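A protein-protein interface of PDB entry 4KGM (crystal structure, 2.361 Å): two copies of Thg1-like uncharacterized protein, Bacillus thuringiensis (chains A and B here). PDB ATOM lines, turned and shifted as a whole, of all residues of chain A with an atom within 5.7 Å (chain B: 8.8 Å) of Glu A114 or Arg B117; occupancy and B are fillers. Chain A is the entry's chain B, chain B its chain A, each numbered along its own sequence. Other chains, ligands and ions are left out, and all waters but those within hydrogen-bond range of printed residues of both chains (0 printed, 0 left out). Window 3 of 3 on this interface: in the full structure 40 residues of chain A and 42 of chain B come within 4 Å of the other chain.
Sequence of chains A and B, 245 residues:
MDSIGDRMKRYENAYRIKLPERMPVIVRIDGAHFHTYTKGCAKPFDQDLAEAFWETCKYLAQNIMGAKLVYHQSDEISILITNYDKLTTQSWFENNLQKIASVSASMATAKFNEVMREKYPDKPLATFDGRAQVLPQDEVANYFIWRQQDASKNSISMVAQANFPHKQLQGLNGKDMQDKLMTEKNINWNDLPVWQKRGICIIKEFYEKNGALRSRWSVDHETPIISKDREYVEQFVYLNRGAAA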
ATOM      1  N   THR A 109     -18.255  -1.327  18.529  1.00  0.00           N
ATOM      2  CA  THR A 109     -18.987  -1.846  19.678  1.00  0.00           C
ATOM      3  C   THR A 109     -20.442  -1.381  19.680  1.00  0.00           C
ATOM      4  O   THR A 109     -21.356  -2.179  19.893  1.00  0.00           O
ATOM      5  CB  THR A 109     -18.321  -1.407  20.996  1.00  0.00           C
ATOM      6  OG1 THR A 109     -16.941  -1.793  20.989  1.00  0.00           O
ATOM      7  CG2 THR A 109     -19.017  -2.038  22.189  1.00  0.00           C
ATOM      8  N   ALA A 110     -20.644  -0.089  19.439  1.00  0.00           N
ATOM      9  CA  ALA A 110     -21.976   0.507  19.471  1.00  0.00           C
ATOM     10  C   ALA A 110     -22.902  -0.097  18.421  1.00  0.00           C
ATOM     11  O   ALA A 110     -24.012  -0.526  18.734  1.00  0.00           O
ATOM     12  CB  ALA A 110     -21.885   2.018  19.288  1.00  0.00           C
ATOM     13  N   LYS A 111     -22.436  -0.130  17.177  1.00  0.00           N
ATOM     14  CA  LYS A 111     -23.244  -0.622  16.069  1.00  0.00           C
ATOM     15  C   LYS A 111     -23.467  -2.130  16.133  1.00  0.00           C
ATOM     16  O   LYS A 111     -24.567  -2.609  15.860  1.00  0.00           O
ATOM     17  CB  LYS A 111     -22.611  -0.232  14.730  1.00  0.00           C
ATOM     18  CG  LYS A 111     -23.300  -0.825  13.508  1.00  0.00           C
ATOM     19  CD  LYS A 111     -24.772  -0.432  13.432  1.00  0.00           C
ATOM     20  CE  LYS A 111     -24.951   1.073  13.305  1.00  0.00           C
ATOM     21  NZ  LYS A 111     -26.380   1.460  13.101  1.00  0.00           N
ATOM     22  N   PHE A 112     -22.426  -2.874  16.495  1.00  0.00           N
ATOM     23  CA  PHE A 112     -22.516  -4.332  16.531  1.00  0.00           C
ATOM     24  C   PHE A 112     -23.517  -4.814  17.579  1.00  0.00           C
ATOM     25  O   PHE A 112     -24.309  -5.715  17.317  1.00  0.00           O
ATOM     26  CB  PHE A 112     -21.142  -4.962  16.783  1.00  0.00           C
ATOM     27  CG  PHE A 112     -21.138  -6.461  16.687  1.00  0.00           C
ATOM     28  CD1 PHE A 112     -20.998  -7.087  15.463  1.00  0.00           C
ATOM     29  CD2 PHE A 112     -21.278  -7.242  17.823  1.00  0.00           C
ATOM     30  CE1 PHE A 112     -20.998  -8.466  15.368  1.00  0.00           C
ATOM     31  CE2 PHE A 112     -21.280  -8.619  17.735  1.00  0.00           C
ATOM     32  CZ  PHE A 112     -21.139  -9.232  16.507  1.00  0.00           C
ATOM     33  N   ASN A 113     -23.476  -4.212  18.762  1.00  0.00           N
ATOM     34  CA  ASN A 113     -24.401  -4.576  19.828  1.00  0.00           C
ATOM     35  C   ASN A 113     -25.841  -4.179  19.513  1.00  0.00           C
ATOM     36  O   ASN A 113     -26.783  -4.868  19.904  1.00  0.00           O
ATOM     37  CB  ASN A 113     -23.961  -3.973  21.163  1.00  0.00           C
ATOM     38  CG  ASN A 113     -22.788  -4.711  21.775  1.00  0.00           C
ATOM     39  OD1 ASN A 113     -22.958  -5.763  22.392  1.00  0.00           O
ATOM     40  ND2 ASN A 113     -21.590  -4.164  21.608  1.00  0.00           N
ATOM     41  N   GLU A 114     -26.005  -3.067  18.803  1.00  0.00           N
ATOM     42  CA  GLU A 114     -27.331  -2.608  18.408  1.00  0.00           C
ATOM     43  C   GLU A 114     -27.972  -3.573  17.413  1.00  0.00           C
ATOM     44  O   GLU A 114     -29.119  -3.987  17.589  1.00  0.00           O
ATOM     45  CB  GLU A 114     -27.257  -1.206  17.803  1.00  0.00           C
ATOM     46  CG  GLU A 114     -28.608  -0.631  17.415  1.00  0.00           C
ATOM     47  CD  GLU A 114     -28.497   0.729  16.754  1.00  0.00           C
ATOM     48  OE1 GLU A 114     -28.931   1.726  17.372  1.00  0.00           O
ATOM     49  OE2 GLU A 114     -27.984   0.800  15.617  1.00  0.00           O
ATOM     50  N   VAL A 115     -27.222  -3.930  16.375  1.00  0.00           N
ATOM     51  CA  VAL A 115     -27.719  -4.810  15.321  1.00  0.00           C
ATOM     52  C   VAL A 115     -27.973  -6.228  15.828  1.00  0.00           C
ATOM     53  O   VAL A 115     -29.000  -6.831  15.518  1.00  0.00           O
ATOM     54  CB  VAL A 115     -26.747  -4.854  14.124  1.00  0.00           C
ATOM     55  CG1 VAL A 115     -27.141  -5.952  13.145  1.00  0.00           C
ATOM     56  CG2 VAL A 115     -26.707  -3.508  13.431  1.00  0.00           C
ATOM     57  N   MET A 116     -27.036  -6.753  16.611  1.00  0.00           N
ATOM     58  CA  MET A 116     -27.165  -8.099  17.160  1.00  0.00           C
ATOM     59  C   MET A 116     -28.356  -8.228  18.106  1.00  0.00           C
ATOM     60  O   MET A 116     -29.100  -9.207  18.044  1.00  0.00           O
ATOM     61  CB  MET A 116     -25.875  -8.526  17.868  1.00  0.00           C
ATOM     62  CG  MET A 116     -24.782  -9.010  16.927  1.00  0.00           C
ATOM     63  SD  MET A 116     -25.127 -10.631  16.202  1.00  0.00           S
ATOM     64  CE  MET A 116     -25.044 -11.679  17.653  1.00  0.00           C
ATOM     65  N   ARG A 117     -28.545  -7.237  18.973  1.00  0.00           N
ATOM     66  CA  ARG A 117     -29.637  -7.289  19.943  1.00  0.00           C
ATOM     67  C   ARG A 117     -31.001  -6.987  19.326  1.00  0.00           C
ATOM     68  O   ARG A 117     -32.014  -6.942  20.023  1.00  0.00           O
ATOM     69  CB  ARG A 117     -29.357  -6.386  21.147  1.00  0.00           C
ATOM     70  CG  ARG A 117     -28.406  -7.024  22.146  1.00  0.00           C
ATOM     71  CD  ARG A 117     -28.350  -6.267  23.456  1.00  0.00           C
ATOM     72  NE  ARG A 117     -27.644  -7.037  24.477  1.00  0.00           N
ATOM     73  CZ  ARG A 117     -27.344  -6.577  25.687  1.00  0.00           C
ATOM     74  NH1 ARG A 117     -27.683  -5.341  26.032  1.00  0.00           N
ATOM     75  NH2 ARG A 117     -26.700  -7.350  26.552  1.00  0.00           N
ATOM     76  N   GLU A 118     -31.018  -6.791  18.013  1.00  0.00           N
ATOM     77  CA  GLU A 118     -32.264  -6.663  17.276  1.00  0.00           C
ATOM     78  C   GLU A 118     -32.809  -8.058  16.975  1.00  0.00           C
ATOM     79  O   GLU A 118     -34.020  -8.279  16.982  1.00  0.00           O
ATOM     80  CB  GLU A 118     -32.040  -5.877  15.984  1.00  0.00           C
ATOM     81  CG  GLU A 118     -33.293  -5.242  15.412  1.00  0.00           C
ATOM     82  CD  GLU A 118     -32.980  -4.094  14.472  1.00  0.00           C
ATOM     83  OE1 GLU A 118     -31.783  -3.853  14.204  1.00  0.00           O
ATOM     84  OE2 GLU A 118     -33.931  -3.429  14.008  1.00  0.00           O
ATOM     85  N   TYR B  37     -25.320  14.718  21.577  1.00  0.00           N
ATOM     86  CA  TYR B  37     -25.960  13.554  22.175  1.00  0.00           C
ATOM     87  C   TYR B  37     -26.822  13.934  23.376  1.00  0.00           C
ATOM     88  O   TYR B  37     -27.885  13.352  23.592  1.00  0.00           O
ATOM     89  CB  TYR B  37     -24.910  12.520  22.588  1.00  0.00           C
ATOM     90  CG  TYR B  37     -25.494  11.264  23.196  1.00  0.00           C
ATOM     91  CD1 TYR B  37     -25.968  10.237  22.390  1.00  0.00           C
ATOM     92  CD2 TYR B  37     -25.566  11.104  24.575  1.00  0.00           C
ATOM     93  CE1 TYR B  37     -26.500   9.089  22.939  1.00  0.00           C
ATOM     94  CE2 TYR B  37     -26.099   9.957  25.133  1.00  0.00           C
ATOM     95  CZ  TYR B  37     -26.563   8.954  24.310  1.00  0.00           C
ATOM     96  OH  TYR B  37     -27.095   7.811  24.854  1.00  0.00           O
ATOM     97  N   ALA B  52     -26.527   6.547  34.188  1.00  0.00           N
ATOM     98  CA  ALA B  52     -26.111   5.652  33.118  1.00  0.00           C
ATOM     99  C   ALA B  52     -24.588   5.568  33.083  1.00  0.00           C
ATOM    100  O   ALA B  52     -24.019   4.527  32.746  1.00  0.00           O
ATOM    101  CB  ALA B  52     -26.652   6.130  31.782  1.00  0.00           C
ATOM    102  N   THR B 109     -18.648   1.936  25.976  1.00  0.00           N
ATOM    103  CA  THR B 109     -19.630   2.056  24.906  1.00  0.00           C
ATOM    104  C   THR B 109     -20.748   1.021  25.027  1.00  0.00           C
ATOM    105  O   THR B 109     -21.926   1.347  24.875  1.00  0.00           O
ATOM    106  CB  THR B 109     -18.960   1.916  23.527  1.00  0.00           C
ATOM    107  OG1 THR B 109     -17.981   2.949  23.363  1.00  0.00           O
ATOM    108  CG2 THR B 109     -19.988   2.019  22.414  1.00  0.00           C
ATOM    109  N   ALA B 110     -20.373  -0.223  25.310  1.00  0.00           N
ATOM    110  CA  ALA B 110     -21.336  -1.321  25.381  1.00  0.00           C
ATOM    111  C   ALA B 110     -22.358  -1.128  26.499  1.00  0.00           C
ATOM    112  O   ALA B 110     -23.567  -1.190  26.267  1.00  0.00           O
ATOM    113  CB  ALA B 110     -20.613  -2.653  25.543  1.00  0.00           C
ATOM    114  N   LYS B 111     -21.868  -0.893  27.711  1.00  0.00           N
ATOM    115  CA  LYS B 111     -22.737  -0.747  28.871  1.00  0.00           C
ATOM    116  C   LYS B 111     -23.604   0.506  28.784  1.00  0.00           C
ATOM    117  O   LYS B 111     -24.807   0.450  29.042  1.00  0.00           O
ATOM    118  CB  LYS B 111     -21.915  -0.745  30.164  1.00  0.00           C
ATOM    119  CG  LYS B 111     -22.730  -0.527  31.438  1.00  0.00           C
ATOM    120  CD  LYS B 111     -23.890  -1.513  31.555  1.00  0.00           C
ATOM    121  CE  LYS B 111     -23.411  -2.956  31.606  1.00  0.00           C
ATOM    122  NZ  LYS B 111     -24.547  -3.922  31.607  1.00  0.00           N
ATOM    123  N   PHE B 112     -22.989   1.625  28.413  1.00  0.00           N
ATOM    124  CA  PHE B 112     -23.686   2.907  28.354  1.00  0.00           C
ATOM    125  C   PHE B 112     -24.857   2.871  27.377  1.00  0.00           C
ATOM    126  O   PHE B 112     -25.979   3.237  27.731  1.00  0.00           O
ATOM    127  CB  PHE B 112     -22.716   4.027  27.971  1.00  0.00           C
ATOM    128  CG  PHE B 112     -23.297   5.404  28.100  1.00  0.00           C
ATOM    129  CD1 PHE B 112     -23.240   6.080  29.308  1.00  0.00           C
ATOM    130  CD2 PHE B 112     -23.892   6.028  27.016  1.00  0.00           C
ATOM    131  CE1 PHE B 112     -23.771   7.349  29.431  1.00  0.00           C
ATOM    132  CE2 PHE B 112     -24.424   7.297  27.135  1.00  0.00           C
ATOM    133  CZ  PHE B 112     -24.362   7.957  28.343  1.00  0.00           C
ATOM    134  N   ASN B 113     -24.592   2.433  26.151  1.00  0.00           N
ATOM    135  CA  ASN B 113     -25.635   2.323  25.140  1.00  0.00           C
ATOM    136  C   ASN B 113     -26.767   1.394  25.575  1.00  0.00           C
ATOM    137  O   ASN B 113     -27.938   1.692  25.350  1.00  0.00           O
ATOM    138  CB  ASN B 113     -25.050   1.863  23.803  1.00  0.00           C
ATOM    139  CG  ASN B 113     -24.455   3.007  23.002  1.00  0.00           C
ATOM    140  OD1 ASN B 113     -25.054   4.077  22.884  1.00  0.00           O
ATOM    141  ND2 ASN B 113     -23.269   2.786  22.445  1.00  0.00           N
ATOM    142  N   GLU B 114     -26.411   0.276  26.204  1.00  0.00           N
ATOM    143  CA  GLU B 114     -27.400  -0.685  26.685  1.00  0.00           C
ATOM    144  C   GLU B 114     -28.364  -0.060  27.690  1.00  0.00           C
ATOM    145  O   GLU B 114     -29.582  -0.155  27.539  1.00  0.00           O
ATOM    146  CB  GLU B 114     -26.716  -1.895  27.324  1.00  0.00           C
ATOM    147  CG  GLU B 114     -27.672  -2.794  28.099  1.00  0.00           C
ATOM    148  CD  GLU B 114     -26.967  -3.927  28.820  1.00  0.00           C
ATOM    149  OE1 GLU B 114     -26.870  -5.033  28.246  1.00  0.00           O
ATOM    150  OE2 GLU B 114     -26.516  -3.715  29.966  1.00  0.00           O
ATOM    151  N   VAL B 115     -27.806   0.574  28.716  1.00  0.00           N
ATOM    152  CA  VAL B 115     -28.600   1.195  29.768  1.00  0.00           C
ATOM    153  C   VAL B 115     -29.438   2.356  29.238  1.00  0.00           C
ATOM    154  O   VAL B 115     -30.614   2.495  29.578  1.00  0.00           O
ATOM    155  CB  VAL B 115     -27.701   1.695  30.922  1.00  0.00           C
ATOM    156  CG1 VAL B 115     -28.496   2.556  31.896  1.00  0.00           C
ATOM    157  CG2 VAL B 115     -27.062   0.517  31.640  1.00  0.00           C
ATOM    158  N   MET B 116     -28.832   3.180  28.393  1.00  0.00           N
ATOM    159  CA  MET B 116     -29.494   4.377  27.893  1.00  0.00           C
ATOM    160  C   MET B 116     -30.667   4.050  26.970  1.00  0.00           C
ATOM    161  O   MET B 116     -31.617   4.825  26.868  1.00  0.00           O
ATOM    162  CB  MET B 116     -28.490   5.284  27.179  1.00  0.00           C
ATOM    163  CG  MET B 116     -28.812   6.759  27.297  1.00  0.00           C
ATOM    164  SD  MET B 116     -28.733   7.352  29.000  1.00  0.00           S
ATOM    165  CE  MET B 116     -29.400   9.000  28.802  1.00  0.00           C
ATOM    166  N   ARG B 117     -30.601   2.902  26.310  1.00  0.00           N
ATOM    167  CA  ARG B 117     -31.669   2.492  25.416  1.00  0.00           C
ATOM    168  C   ARG B 117     -32.954   2.328  26.214  1.00  0.00           C
ATOM    169  O   ARG B 117     -34.042   2.655  25.741  1.00  0.00           O
ATOM    170  CB  ARG B 117     -31.311   1.181  24.715  1.00  0.00           C
ATOM    171  CG  ARG B 117     -30.499   1.360  23.442  1.00  0.00           C
ATOM    172  CD  ARG B 117     -30.979   2.561  22.646  1.00  0.00           C
ATOM    173  NE  ARG B 117     -30.648   2.446  21.228  1.00  0.00           N
ATOM    174  CZ  ARG B 117     -29.759   3.213  20.604  1.00  0.00           C
ATOM    175  NH1 ARG B 117     -28.914   3.957  21.304  1.00  0.00           N
ATOM    176  NH2 ARG B 117     -29.715   3.235  19.279  1.00  0.00           N
ATOM    177  N   GLU B 118     -32.815   1.804  27.426  1.00  0.00           N
ATOM    178  CA  GLU B 118     -33.962   1.417  28.240  1.00  0.00           C
ATOM    179  C   GLU B 118     -34.994   2.538  28.305  1.00  0.00           C
ATOM    180  O   GLU B 118     -36.173   2.328  28.019  1.00  0.00           O
ATOM    181  CB  GLU B 118     -33.521   1.049  29.659  1.00  0.00           C
ATOM    182  CG  GLU B 118     -32.544  -0.110  29.741  1.00  0.00           C
ATOM    183  CD  GLU B 118     -32.101  -0.395  31.166  1.00  0.00           C
ATOM    184  OE1 GLU B 118     -31.097  -1.117  31.345  1.00  0.00           O
ATOM    185  OE2 GLU B 118     -32.758   0.103  32.106  1.00  0.00           O
ATOM    186  N   LYS B 119     -34.541   3.728  28.682  1.00  0.00           N
ATOM    187  CA  LYS B 119     -35.433   4.869  28.851  1.00  0.00           C
ATOM    188  C   LYS B 119     -35.402   5.804  27.647  1.00  0.00           C
ATOM    189  O   LYS B 119     -36.254   6.683  27.513  1.00  0.00           O
ATOM    190  CB  LYS B 119     -35.075   5.643  30.122  1.00  0.00           C
ATOM    191  N   TYR B 120     -34.416   5.620  26.776  1.00  0.00           N
ATOM    192  CA  TYR B 120     -34.275   6.481  25.607  1.00  0.00           C
ATOM    193  C   TYR B 120     -33.886   5.698  24.356  1.00  0.00           C
ATOM    194  O   TYR B 120     -32.788   5.878  23.832  1.00  0.00           O
ATOM    195  CB  TYR B 120     -33.234   7.571  25.873  1.00  0.00           C
ATOM    196  CG  TYR B 120     -33.531   8.428  27.083  1.00  0.00           C
ATOM    197  CD1 TYR B 120     -33.051   8.080  28.341  1.00  0.00           C
ATOM    198  CD2 TYR B 120     -34.289   9.586  26.968  1.00  0.00           C
ATOM    199  CE1 TYR B 120     -33.322   8.860  29.449  1.00  0.00           C
ATOM    200  CE2 TYR B 120     -34.563  10.372  28.072  1.00  0.00           C
ATOM    201  CZ  TYR B 120     -34.077  10.005  29.308  1.00  0.00           C
ATOM    202  OH  TYR B 120     -34.348  10.785  30.407  1.00  0.00           O
ATOM    203  N   PRO B 121     -34.791   4.837  23.863  1.00  0.00           N
ATOM    204  CA  PRO B 121     -34.470   4.025  22.684  1.00  0.00           C
ATOM    205  C   PRO B 121     -34.383   4.855  21.406  1.00  0.00           C
ATOM    206  O   PRO B 121     -33.937   4.349  20.374  1.00  0.00           O
ATOM    207  CB  PRO B 121     -35.644   3.044  22.608  1.00  0.00           C
ATOM    208  CG  PRO B 121     -36.771   3.758  23.264  1.00  0.00           C
ATOM    209  CD  PRO B 121     -36.154   4.578  24.360  1.00  0.00           C
ATOM    210  N   ASP B 122     -34.803   6.114  21.478  1.00  0.00           N
ATOM    211  CA  ASP B 122     -34.761   7.004  20.324  1.00  0.00           C
ATOM    212  C   ASP B 122     -33.410   7.707  20.210  1.00  0.00           C
ATOM    213  O   ASP B 122     -33.061   8.233  19.151  1.00  0.00           O
ATOM    214  CB  ASP B 122     -35.890   8.035  20.401  1.00  0.00           C
ATOM    215  N   LYS B 123     -32.658   7.714  21.307  1.00  0.00           N
ATOM    216  CA  LYS B 123     -31.328   8.314  21.331  1.00  0.00           C
ATOM    217  C   LYS B 123     -30.419   7.624  20.318  1.00  0.00           C
ATOM    218  O   LYS B 123     -30.462   6.403  20.176  1.00  0.00           O
ATOM    219  CB  LYS B 123     -30.715   8.190  22.727  1.00  0.00           C
ATOM    220  CG  LYS B 123     -30.162   9.486  23.302  1.00  0.00           C
ATOM    221  CD  LYS B 123     -31.238  10.274  24.031  1.00  0.00           C
ATOM    222  CE  LYS B 123     -30.652  11.470  24.766  1.00  0.00           C
ATOM    223  NZ  LYS B 123     -31.676  12.193  25.572  1.00  0.00           N
ATOM    224  N   PRO B 124     -29.598   8.407  19.601  1.00  0.00           N
ATOM    225  CA  PRO B 124     -28.635   7.821  18.663  1.00  0.00           C
ATOM    226  C   PRO B 124     -27.516   7.098  19.409  1.00  0.00           C
ATOM    227  O   PRO B 124     -27.437   7.178  20.636  1.00  0.00           O
ATOM    228  CB  PRO B 124     -28.083   9.040  17.919  1.00  0.00           C
ATOM    229  CG  PRO B 124     -28.267  10.175  18.868  1.00  0.00           C
ATOM    230  CD  PRO B 124     -29.534   9.879  19.617  1.00  0.00           C
ATOM    231  N   LEU B 125     -26.661   6.397  18.676  1.00  0.00           N
ATOM    232  CA  LEU B 125     -25.573   5.651  19.298  1.00  0.00           C
ATOM    233  C   LEU B 125     -24.546   6.575  19.942  1.00  0.00           C
ATOM    234  O   LEU B 125     -24.087   7.539  19.327  1.00  0.00           O
ATOM    235  CB  LEU B 125     -24.901   4.733  18.276  1.00  0.00           C
ATOM    236  CG  LEU B 125     -25.773   3.577  17.786  1.00  0.00           C
ATOM    237  CD1 LEU B 125     -25.051   2.765  16.723  1.00  0.00           C
ATOM    238  CD2 LEU B 125     -26.179   2.700  18.961  1.00  0.00           C
ATOM    239  N   ALA B 126     -24.199   6.277  21.190  1.00  0.00           N
ATOM    240  CA  ALA B 126     -23.170   7.027  21.899  1.00  0.00           C
ATOM    241  C   ALA B 126     -21.814   6.366  21.701  1.00  0.00           C
ATOM    242  O   ALA B 126     -21.700   5.140  21.744  1.00  0.00           O
ATOM    243  CB  ALA B 126     -23.504   7.118  23.379  1.00  0.00           C
ATOM    244  N   THR B 127     -20.788   7.180  21.471  1.00  0.00           N
ATOM    245  CA  THR B 127     -19.429   6.672  21.325  1.00  0.00           C
ATOM    246  C   THR B 127     -18.472   7.368  22.285  1.00  0.00           C
ATOM    247  O   THR B 127     -18.761   8.453  22.793  1.00  0.00           O
ATOM    248  CB  THR B 127     -18.909   6.822  19.882  1.00  0.00           C
ATOM    249  OG1 THR B 127     -19.050   8.183  19.459  1.00  0.00           O
ATOM    250  CG2 THR B 127     -19.687   5.916  18.939  1.00  0.00           C
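The backbone carbonyl oxygen (O) of Thr B109 is in hydrogen-bond range of the side-chain amide nitrogen (ND2) of Asn B113. NZ of Lys B111 is in salt-bridge range of OE2 of Glu B114. The guanidinium group (NH1) of Arg B117 lies within hydrogen-bond range of the backbone carbonyl oxygen (O) of Lys B123. The side-chain carboxylate (OE2) of Glu A114 is in salt-bridge range of the side-chain amino group (NZ) of Lys A111 (3.1 Å). The backbone NH (N) of Ala B126 is in hydrogen-bond range of the side-chain amide oxygen (OD1) of Asn B113, at 2.9 Å. The backbone carbonyl oxygen (O) of Thr A109 lies within hydrogen-bond range of the side-chain amide nitrogen (ND2) of Asn A113 (2.6 Å).
Among the printed residues, merely in contact across the chains: Glu A114 with Leu B125 (3.3 Å), Ala A110 with Asn B113 (3.5 Å), Ala A110 with Thr B109 (3.7 Å), Thr A109 with Ala B110 (3.8 Å), Lys A111 with Leu B125 (3.8 Å), Ala A110 with Leu B125 (3.9 Å) and Ala A110 with Ala B126 (3.98 Å).
Thr A109 touches Ala B110, and with the chains exchanged Ala A110 touches Thr B109. Ala A110 touches Asn B113, but with the chains exchanged Asn A113 does not touch Ala B110 (4.3 Å). Glu A114 touches Arg B117, and with the chains exchanged Arg A117 touches Glu B114. Positions printed for both chains: 109, 110, 111, 112, 113, 114, 115, 116, 117 and 118. Of the 9 pairs that touch across the chains among the printed residues, 4 have their exchanged pair printed and touching as well.
NH2 of Arg A117 lies within salt-bridge range of OE1 of Glu B114, 2.9 Å away. The guanidinium group (NH2) of Arg B117 lies within salt-bridge range of the side-chain carboxylate (OE1) of Glu A114.
Of the printed residues of chain B, Thr A109 touches Ala B110. Of chain B, only Arg B117 and Leu B125 come within 4 Å of Glu A114. Of the printed residues of chain A, Thr B109 touches Ala A110 (3.7 Å). Lys B111 touches none of the printed residues of chain A. Of the printed residues of chain A, Asn B113 touches Ala A110 (3.5 Å). Of the printed residues of chain A, Glu B114 touches Arg A117 (2.4 Å). Met B116 touches none of the printed residues of chain A. Of the printed residues of chain A, Arg B117 touches Glu A114 (2.6 Å). The nearest residue of chain B that does not touch Glu A114 is Lys B123 (5.7 Å). The nearest printed residue of chain A that does not touch Arg B117 is Ala A110 (6.9 Å). The nearest printed residue of chain A that does not touch Leu B125 is Phe A112 (6.2 Å).
Hydrophobic or aromatic side chains of chain A that line the printed part of chain B: Ala A110. Along chain A the printed residues that touch a printed residue of chain B span positions 109 to 117. Of the 21 printed residues of chain B, 7 touch a printed residue of chain A. Hydrophobic or aromatic side chains of chain B within 4 Å of the printed part of chain A: Ala B110 and Leu B125. Among the printed residues, 9 pairs touch across the chains. Among the printed residues, Asp or Glu carboxylates within 4 Å of a Lys or Arg side-chain nitrogen of the other chain: Glu A114 with Arg B117 (2.6 Å) and Arg A117 with Glu B114 (2.4 Å).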
